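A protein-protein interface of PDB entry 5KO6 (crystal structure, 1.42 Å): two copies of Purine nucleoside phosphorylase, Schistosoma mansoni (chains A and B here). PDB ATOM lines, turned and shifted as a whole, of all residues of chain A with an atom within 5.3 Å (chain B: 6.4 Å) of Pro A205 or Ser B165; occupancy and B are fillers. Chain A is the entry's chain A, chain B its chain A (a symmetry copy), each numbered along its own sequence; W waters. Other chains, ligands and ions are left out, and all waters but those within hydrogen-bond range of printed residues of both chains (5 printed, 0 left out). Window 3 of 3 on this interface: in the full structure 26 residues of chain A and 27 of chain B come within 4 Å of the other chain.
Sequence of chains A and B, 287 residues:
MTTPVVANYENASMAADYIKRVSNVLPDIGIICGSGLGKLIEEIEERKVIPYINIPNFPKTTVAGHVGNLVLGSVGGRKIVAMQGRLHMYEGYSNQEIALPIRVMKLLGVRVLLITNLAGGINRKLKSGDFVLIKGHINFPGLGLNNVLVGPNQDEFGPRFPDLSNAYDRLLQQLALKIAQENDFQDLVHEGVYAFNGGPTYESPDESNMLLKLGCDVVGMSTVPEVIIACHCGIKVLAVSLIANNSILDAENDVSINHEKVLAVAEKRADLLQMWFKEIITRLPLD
OD1 of Asp A254 is in salt-bridge range of NH2 of Arg B170 (3.5 Å). The side-chain hydroxyl of Ser A204 lies within hydrogen-bond range of the backbone carbonyl oxygen of His B137, 2.9 Å away. The side-chain carboxylate of Asp A254 lies within hydrogen-bond range of the side-chain amide nitrogen of Asn B166, 3.5 Å away.
OD1 of Asp B163 lies within hydrogen-bond range of N of Ser B165, at 2.7 Å. The side-chain carboxylate of Glu A207 lies within hydrogen-bond range of the backbone NH of Ser A204 (2.9 Å). The backbone carbonyl oxygen of Asp B163 is in hydrogen-bond range of the side-chain sulfur of Cys B231 (3.6 Å). ND1 of His B137 is in hydrogen-bond range of OH of Tyr B168 (2.8 Å). The backbone carbonyl oxygen of Ser A204 lies within hydrogen-bond range of the side-chain hydroxyl of Ser A208, 3.2 Å away.
Pro A205 touches Ser B165 (CG to CB, 3.7 Å). Asp A206 touches His B137 (CB to O, 3.7 Å). His B137 touches Glu A207 (CD2 to OE2, 3.6 Å). Asp B163 touches Ser A256 (OD2 to CA, 3.7 Å).
Of chain B, only Ser B165 (3.7 Å) comes within 4 Å of Pro A205. Met A210 touches none of the printed residues of chain B. Lys B135 touches none of the printed residues of chain A. Ser B165 touches just one residue of chain A: Pro A205 (3.7 Å). Printed residues of chain A within 4 Å of Asn B166: Asp A254 (3.5 Å). Of the printed residues of chain A, Arg B170 touches Asp A254.
Of the 10 printed residues of chain B, 5 touch a printed residue of chain A. Along chain A the printed residues that touch a printed residue of chain B span positions 204 to 256. Among the printed residues, 7 pairs touch across the chains.
No position is printed for both chains. Of the 7 pairs that touch across the chains among the printed residues, none has its exchanged pair printed and touching as well.
Water W3 lies within hydrogen-bond range of OD1 of Asn B166, OD1 of Asp A254 and OG of Ser B165. Water W5 lies within hydrogen-bond range of the side-chain carboxylate (OD2) of Asp A206, the backbone NH (N) of His B137 and the side-chain hydroxyl (OG) of Ser A204. Water W1 lies within hydrogen-bond range of the backbone NH of Leu B164 and the backbone carbonyl oxygen of Glu A203. Water W4 bridges the side-chain carboxylate (OE2) of Glu A207 (2.7 Å) and a ring nitrogen (NE2) of His B137 (2.8 Å). Water W2 bridges the side-chain carboxylate (OD2) of Asp B163 (2.9 Å) and the backbone carbonyl oxygen (O) of Glu A203 (3.2 Å).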
ATOM      1  N   GLU A 203     -10.300  26.871   7.841  1.00  0.00           N
ATOM      2  CA  GLU A 203     -11.559  26.169   7.633  1.00  0.00           C
ATOM      3  C   GLU A 203     -11.931  25.424   8.909  1.00  0.00           C
ATOM      4  O   GLU A 203     -11.088  24.774   9.533  1.00  0.00           O
ATOM      5  CB  GLU A 203     -11.389  25.177   6.460  1.00  0.00           C
ATOM      6  CG  GLU A 203     -10.377  23.993   6.650  1.00  0.00           C
ATOM      7  CD  GLU A 203      -8.909  24.330   6.431  1.00  0.00           C
ATOM      8  OE1 GLU A 203      -8.569  25.502   6.224  1.00  0.00           O
ATOM      9  OE2 GLU A 203      -8.059  23.406   6.469  1.00  0.00           O
ATOM     10  N   SER A 204     -13.188  25.582   9.335  1.00  0.00           N
ATOM     11  CA  SER A 204     -13.665  24.870  10.508  1.00  0.00           C
ATOM     12  C   SER A 204     -13.834  23.394  10.165  1.00  0.00           C
ATOM     13  O   SER A 204     -13.915  23.033   8.988  1.00  0.00           O
ATOM     14  CB  SER A 204     -15.011  25.434  10.945  1.00  0.00           C
ATOM     15  OG  SER A 204     -16.040  25.019  10.059  1.00  0.00           O
ATOM     16  N   PRO A 205     -13.875  22.518  11.178  1.00  0.00           N
ATOM     17  CA  PRO A 205     -14.059  21.087  10.879  1.00  0.00           C
ATOM     18  C   PRO A 205     -15.285  20.804  10.024  1.00  0.00           C
ATOM     19  O   PRO A 205     -15.230  19.977   9.103  1.00  0.00           O
ATOM     20  CB  PRO A 205     -14.168  20.447  12.272  1.00  0.00           C
ATOM     21  CG  PRO A 205     -13.409  21.365  13.171  1.00  0.00           C
ATOM     22  CD  PRO A 205     -13.610  22.763  12.609  1.00  0.00           C
ATOM     23  N   ASP A 206     -16.393  21.489  10.297  1.00  0.00           N
ATOM     24  CA  ASP A 206     -17.598  21.279   9.511  1.00  0.00           C
ATOM     25  C   ASP A 206     -17.488  21.895   8.127  1.00  0.00           C
ATOM     26  O   ASP A 206     -18.033  21.339   7.168  1.00  0.00           O
ATOM     27  CB  ASP A 206     -18.797  21.768  10.307  1.00  0.00           C
ATOM     28  CG  ASP A 206     -18.982  20.952  11.564  1.00  0.00           C
ATOM     29  OD1 ASP A 206     -19.327  19.752  11.442  1.00  0.00           O
ATOM     30  OD2 ASP A 206     -18.730  21.473  12.669  1.00  0.00           O
ATOM     31  N   GLU A 207     -16.745  22.993   7.984  1.00  0.00           N
ATOM     32  CA  GLU A 207     -16.471  23.495   6.642  1.00  0.00           C
ATOM     33  C   GLU A 207     -15.617  22.509   5.854  1.00  0.00           C
ATOM     34  O   GLU A 207     -15.852  22.289   4.660  1.00  0.00           O
ATOM     35  CB  GLU A 207     -15.792  24.861   6.720  1.00  0.00           C
ATOM     36  CG  GLU A 207     -16.774  25.960   7.157  1.00  0.00           C
ATOM     37  CD  GLU A 207     -16.093  27.182   7.769  1.00  0.00           C
ATOM     38  OE1 GLU A 207     -14.848  27.287   7.727  1.00  0.00           O
ATOM     39  OE2 GLU A 207     -16.807  28.039   8.325  1.00  0.00           O
ATOM     40  N   SER A 208     -14.630  21.891   6.508  1.00  0.00           N
ATOM     41  CA  SER A 208     -13.813  20.901   5.820  1.00  0.00           C
ATOM     42  C   SER A 208     -14.673  19.759   5.310  1.00  0.00           C
ATOM     43  O   SER A 208     -14.513  19.308   4.168  1.00  0.00           O
ATOM     44  CB  SER A 208     -12.749  20.365   6.775  1.00  0.00           C
ATOM     45  OG  SER A 208     -11.868  21.414   7.122  1.00  0.00           O
ATOM     46  N   ASN A 209     -15.587  19.273   6.154  1.00  0.00           N
ATOM     47  CA  ASN A 209     -16.462  18.185   5.738  1.00  0.00           C
ATOM     48  C   ASN A 209     -17.322  18.611   4.559  1.00  0.00           C
ATOM     49  O   ASN A 209     -17.558  17.825   3.634  1.00  0.00           O
ATOM     50  CB  ASN A 209     -17.345  17.750   6.908  1.00  0.00           C
ATOM     51  CG  ASN A 209     -16.582  16.977   7.961  1.00  0.00           C
ATOM     52  OD1 ASN A 209     -15.546  16.377   7.678  1.00  0.00           O
ATOM     53  ND2 ASN A 209     -17.094  16.983   9.189  1.00  0.00           N
ATOM     54  N   MET A 210     -17.793  19.859   4.570  1.00  0.00           N
ATOM     55  CA  MET A 210     -18.565  20.354   3.438  1.00  0.00           C
ATOM     56  C   MET A 210     -17.719  20.382   2.172  1.00  0.00           C
ATOM     57  O   MET A 210     -18.178  19.963   1.102  1.00  0.00           O
ATOM     58  CB  MET A 210     -19.106  21.748   3.753  1.00  0.00           C
ATOM     59  CG  MET A 210     -19.742  22.392   2.554  1.00  0.00           C
ATOM     60  SD  MET A 210     -20.349  24.043   2.909  1.00  0.00           S
ATOM     61  CE  MET A 210     -18.849  24.949   2.904  1.00  0.00           C
ATOM     62  N   ALA A 251     -10.166  16.788  11.637  1.00  0.00           N
ATOM     63  CA  ALA A 251     -11.522  16.881  12.175  1.00  0.00           C
ATOM     64  C   ALA A 251     -11.927  15.579  12.843  1.00  0.00           C
ATOM     65  O   ALA A 251     -12.554  15.585  13.911  1.00  0.00           O
ATOM     66  CB  ALA A 251     -12.507  17.243  11.063  1.00  0.00           C
ATOM     67  N   ASP A 254      -9.745  15.412  16.178  1.00  0.00           N
ATOM     68  CA  ASP A 254      -9.705  16.585  17.054  1.00  0.00           C
ATOM     69  C   ASP A 254      -8.285  17.136  17.188  1.00  0.00           C
ATOM     70  O   ASP A 254      -7.797  17.418  18.285  1.00  0.00           O
ATOM     71  CB  ASP A 254     -10.340  16.303  18.419  1.00  0.00           C
ATOM     72  CG  ASP A 254     -10.679  17.573  19.177  1.00  0.00           C
ATOM     73  OD1 ASP A 254     -11.002  18.596  18.528  1.00  0.00           O
ATOM     74  OD2 ASP A 254     -10.619  17.549  20.425  1.00  0.00           O
ATOM     75  N   VAL A 255      -7.619  17.288  16.055  1.00  0.00           N
ATOM     76  CA  VAL A 255      -6.276  17.848  16.002  1.00  0.00           C
ATOM     77  C   VAL A 255      -6.367  19.273  15.472  1.00  0.00           C
ATOM     78  O   VAL A 255      -7.074  19.542  14.494  1.00  0.00           O
ATOM     79  CB  VAL A 255      -5.363  16.966  15.129  1.00  0.00           C
ATOM     80  CG1 VAL A 255      -4.063  17.694  14.785  1.00  0.00           C
ATOM     81  CG2 VAL A 255      -5.072  15.634  15.838  1.00  0.00           C
ATOM     82  N   SER A 256      -5.660  20.191  16.123  1.00  0.00           N
ATOM     83  CA  SER A 256      -5.740  21.593  15.749  1.00  0.00           C
ATOM     84  C   SER A 256      -4.718  21.915  14.666  1.00  0.00           C
ATOM     85  O   SER A 256      -3.793  21.149  14.389  1.00  0.00           O
ATOM     86  CB  SER A 256      -5.492  22.480  16.967  1.00  0.00           C
ATOM     87  OG  SER A 256      -4.161  22.326  17.423  1.00  0.00           O
ATOM     88  N   LYS B 135     -22.288  23.014  18.066  1.00  0.00           N
ATOM     89  CA  LYS B 135     -21.019  22.316  18.215  1.00  0.00           C
ATOM     90  C   LYS B 135     -20.025  22.639  17.113  1.00  0.00           C
ATOM     91  O   LYS B 135     -18.874  22.198  17.200  1.00  0.00           O
ATOM     92  CB  LYS B 135     -21.235  20.792  18.279  1.00  0.00           C
ATOM     93  CG  LYS B 135     -21.777  20.198  16.987  1.00  0.00           C
ATOM     94  CD  LYS B 135     -21.925  18.685  17.092  1.00  0.00           C
ATOM     95  CE  LYS B 135     -22.464  18.100  15.796  1.00  0.00           C
ATOM     96  NZ  LYS B 135     -22.663  16.627  15.894  1.00  0.00           N
ATOM     97  N   HIS B 137     -19.733  25.167  13.021  1.00  0.00           N
ATOM     98  CA  HIS B 137     -20.455  26.049  12.112  1.00  0.00           C
ATOM     99  C   HIS B 137     -19.951  25.948  10.675  1.00  0.00           C
ATOM    100  O   HIS B 137     -18.849  25.458  10.396  1.00  0.00           O
ATOM    101  CB  HIS B 137     -20.458  27.507  12.592  1.00  0.00           C
ATOM    102  CG  HIS B 137     -19.110  28.164  12.587  1.00  0.00           C
ATOM    103  ND1 HIS B 137     -18.606  28.814  13.689  1.00  0.00           N
ATOM    104  CD2 HIS B 137     -18.181  28.304  11.607  1.00  0.00           C
ATOM    105  CE1 HIS B 137     -17.425  29.325  13.397  1.00  0.00           C
ATOM    106  NE2 HIS B 137     -17.141  29.029  12.140  1.00  0.00           N
ATOM    107  N   ASP B 163      -7.576  28.965  14.771  1.00  0.00           N
ATOM    108  CA  ASP B 163      -8.185  27.659  14.553  1.00  0.00           C
ATOM    109  C   ASP B 163      -9.507  27.648  15.308  1.00  0.00           C
ATOM    110  O   ASP B 163      -9.558  28.021  16.488  1.00  0.00           O
ATOM    111  CB  ASP B 163      -7.280  26.552  15.098  1.00  0.00           C
ATOM    112  CG  ASP B 163      -7.911  25.169  14.970  1.00  0.00           C
ATOM    113  OD1 ASP B 163      -8.815  24.843  15.763  1.00  0.00           O
ATOM    114  OD2 ASP B 163      -7.491  24.400  14.086  1.00  0.00           O
ATOM    115  N   LEU B 164     -10.581  27.242  14.627  1.00  0.00           N
ATOM    116  CA  LEU B 164     -11.915  27.262  15.206  1.00  0.00           C
ATOM    117  C   LEU B 164     -12.409  25.882  15.625  1.00  0.00           C
ATOM    118  O   LEU B 164     -13.577  25.743  16.015  1.00  0.00           O
ATOM    119  CB  LEU B 164     -12.901  27.895  14.224  1.00  0.00           C
ATOM    120  CG  LEU B 164     -12.564  29.292  13.737  1.00  0.00           C
ATOM    121  CD1 LEU B 164     -13.579  29.697  12.671  1.00  0.00           C
ATOM    122  CD2 LEU B 164     -12.562  30.309  14.876  1.00  0.00           C
ATOM    123  N   SER B 165     -11.553  24.863  15.563  1.00  0.00           N
ATOM    124  CA  SER B 165     -11.995  23.512  15.884  1.00  0.00           C
ATOM    125  C   SER B 165     -12.439  23.363  17.333  1.00  0.00           C
ATOM    126  O   SER B 165     -13.219  22.452  17.631  1.00  0.00           O
ATOM    127  CB  SER B 165     -10.894  22.511  15.561  1.00  0.00           C
ATOM    128  OG  SER B 165      -9.740  22.787  16.323  1.00  0.00           O
ATOM    129  N   ASN B 166     -11.985  24.246  18.229  1.00  0.00           N
ATOM    130  CA  ASN B 166     -12.411  24.258  19.624  1.00  0.00           C
ATOM    131  C   ASN B 166     -13.148  25.544  19.999  1.00  0.00           C
ATOM    132  O   ASN B 166     -13.150  25.955  21.159  1.00  0.00           O
ATOM    133  CB  ASN B 166     -11.219  23.975  20.537  1.00  0.00           C
ATOM    134  CG  ASN B 166     -10.628  22.612  20.271  1.00  0.00           C
ATOM    135  OD1 ASN B 166      -9.415  22.459  20.114  1.00  0.00           O
ATOM    136  ND2 ASN B 166     -11.505  21.605  20.163  1.00  0.00           N
ATOM    137  N   ALA B 167     -13.822  26.175  19.034  1.00  0.00           N
ATOM    138  CA  ALA B 167     -14.484  27.453  19.314  1.00  0.00           C
ATOM    139  C   ALA B 167     -15.689  27.297  20.240  1.00  0.00           C
ATOM    140  O   ALA B 167     -16.016  28.226  20.991  1.00  0.00           O
ATOM    141  CB  ALA B 167     -14.908  28.125  18.011  1.00  0.00           C
ATOM    142  N   TYR B 168     -16.370  26.155  20.190  1.00  0.00           N
ATOM    143  CA  TYR B 168     -17.546  25.878  21.014  1.00  0.00           C
ATOM    144  C   TYR B 168     -17.116  24.895  22.096  1.00  0.00           C
ATOM    145  O   TYR B 168     -16.987  23.698  21.833  1.00  0.00           O
ATOM    146  CB  TYR B 168     -18.675  25.315  20.154  1.00  0.00           C
ATOM    147  CG  TYR B 168     -19.072  26.253  19.042  1.00  0.00           C
ATOM    148  CD1 TYR B 168     -20.003  27.266  19.260  1.00  0.00           C
ATOM    149  CD2 TYR B 168     -18.497  26.160  17.771  1.00  0.00           C
ATOM    150  CE1 TYR B 168     -20.369  28.151  18.256  1.00  0.00           C
ATOM    151  CE2 TYR B 168     -18.858  27.051  16.751  1.00  0.00           C
ATOM    152  CZ  TYR B 168     -19.788  28.043  17.003  1.00  0.00           C
ATOM    153  OH  TYR B 168     -20.166  28.928  16.033  1.00  0.00           O
ATOM    154  N   ARG B 170     -16.545  22.225  24.759  1.00  0.00           N
ATOM    155  CA  ARG B 170     -17.278  20.979  24.957  1.00  0.00           C
ATOM    156  C   ARG B 170     -17.818  20.856  26.379  1.00  0.00           C
ATOM    157  O   ARG B 170     -18.958  20.419  26.574  1.00  0.00           O
ATOM    158  CB  ARG B 170     -16.409  19.780  24.578  1.00  0.00           C
ATOM    159  CG  ARG B 170     -16.471  19.446  23.090  1.00  0.00           C
ATOM    160  CD  ARG B 170     -15.817  18.105  22.793  1.00  0.00           C
ATOM    161  NE  ARG B 170     -14.363  18.214  22.774  1.00  0.00           N
ATOM    162  CZ  ARG B 170     -13.634  18.256  21.664  1.00  0.00           C
ATOM    163  NH1 ARG B 170     -14.222  18.183  20.478  1.00  0.00           N
ATOM    164  NH2 ARG B 170     -12.315  18.365  21.742  1.00  0.00           N
ATOM    165  N   CYS B 231     -13.239  33.619  20.100  1.00  0.00           N
ATOM    166  CA  CYS B 231     -12.212  32.589  19.969  1.00  0.00           C
ATOM    167  C   CYS B 231     -10.845  33.217  19.710  1.00  0.00           C
ATOM    168  O   CYS B 231      -9.833  32.799  20.281  1.00  0.00           O
ATOM    169  CB  CYS B 231     -12.598  31.651  18.829  1.00  0.00           C
ATOM    170  SG  CYS B 231     -11.470  30.262  18.571  1.00  0.00           S
HETATM  171  O   HOH W   1     -10.858  26.342  12.079  1.00  0.00           O
HETATM  172  O   HOH W   2      -9.646  23.842  12.209  1.00  0.00           O
HETATM  173  O   HOH W   3      -8.453  20.594  18.437  1.00  0.00           O
HETATM  174  O   HOH W   4     -15.540  29.844   9.949  1.00  0.00           O
HETATM  175  O   HOH W   5     -17.122  23.656  12.674  1.00  0.00           O
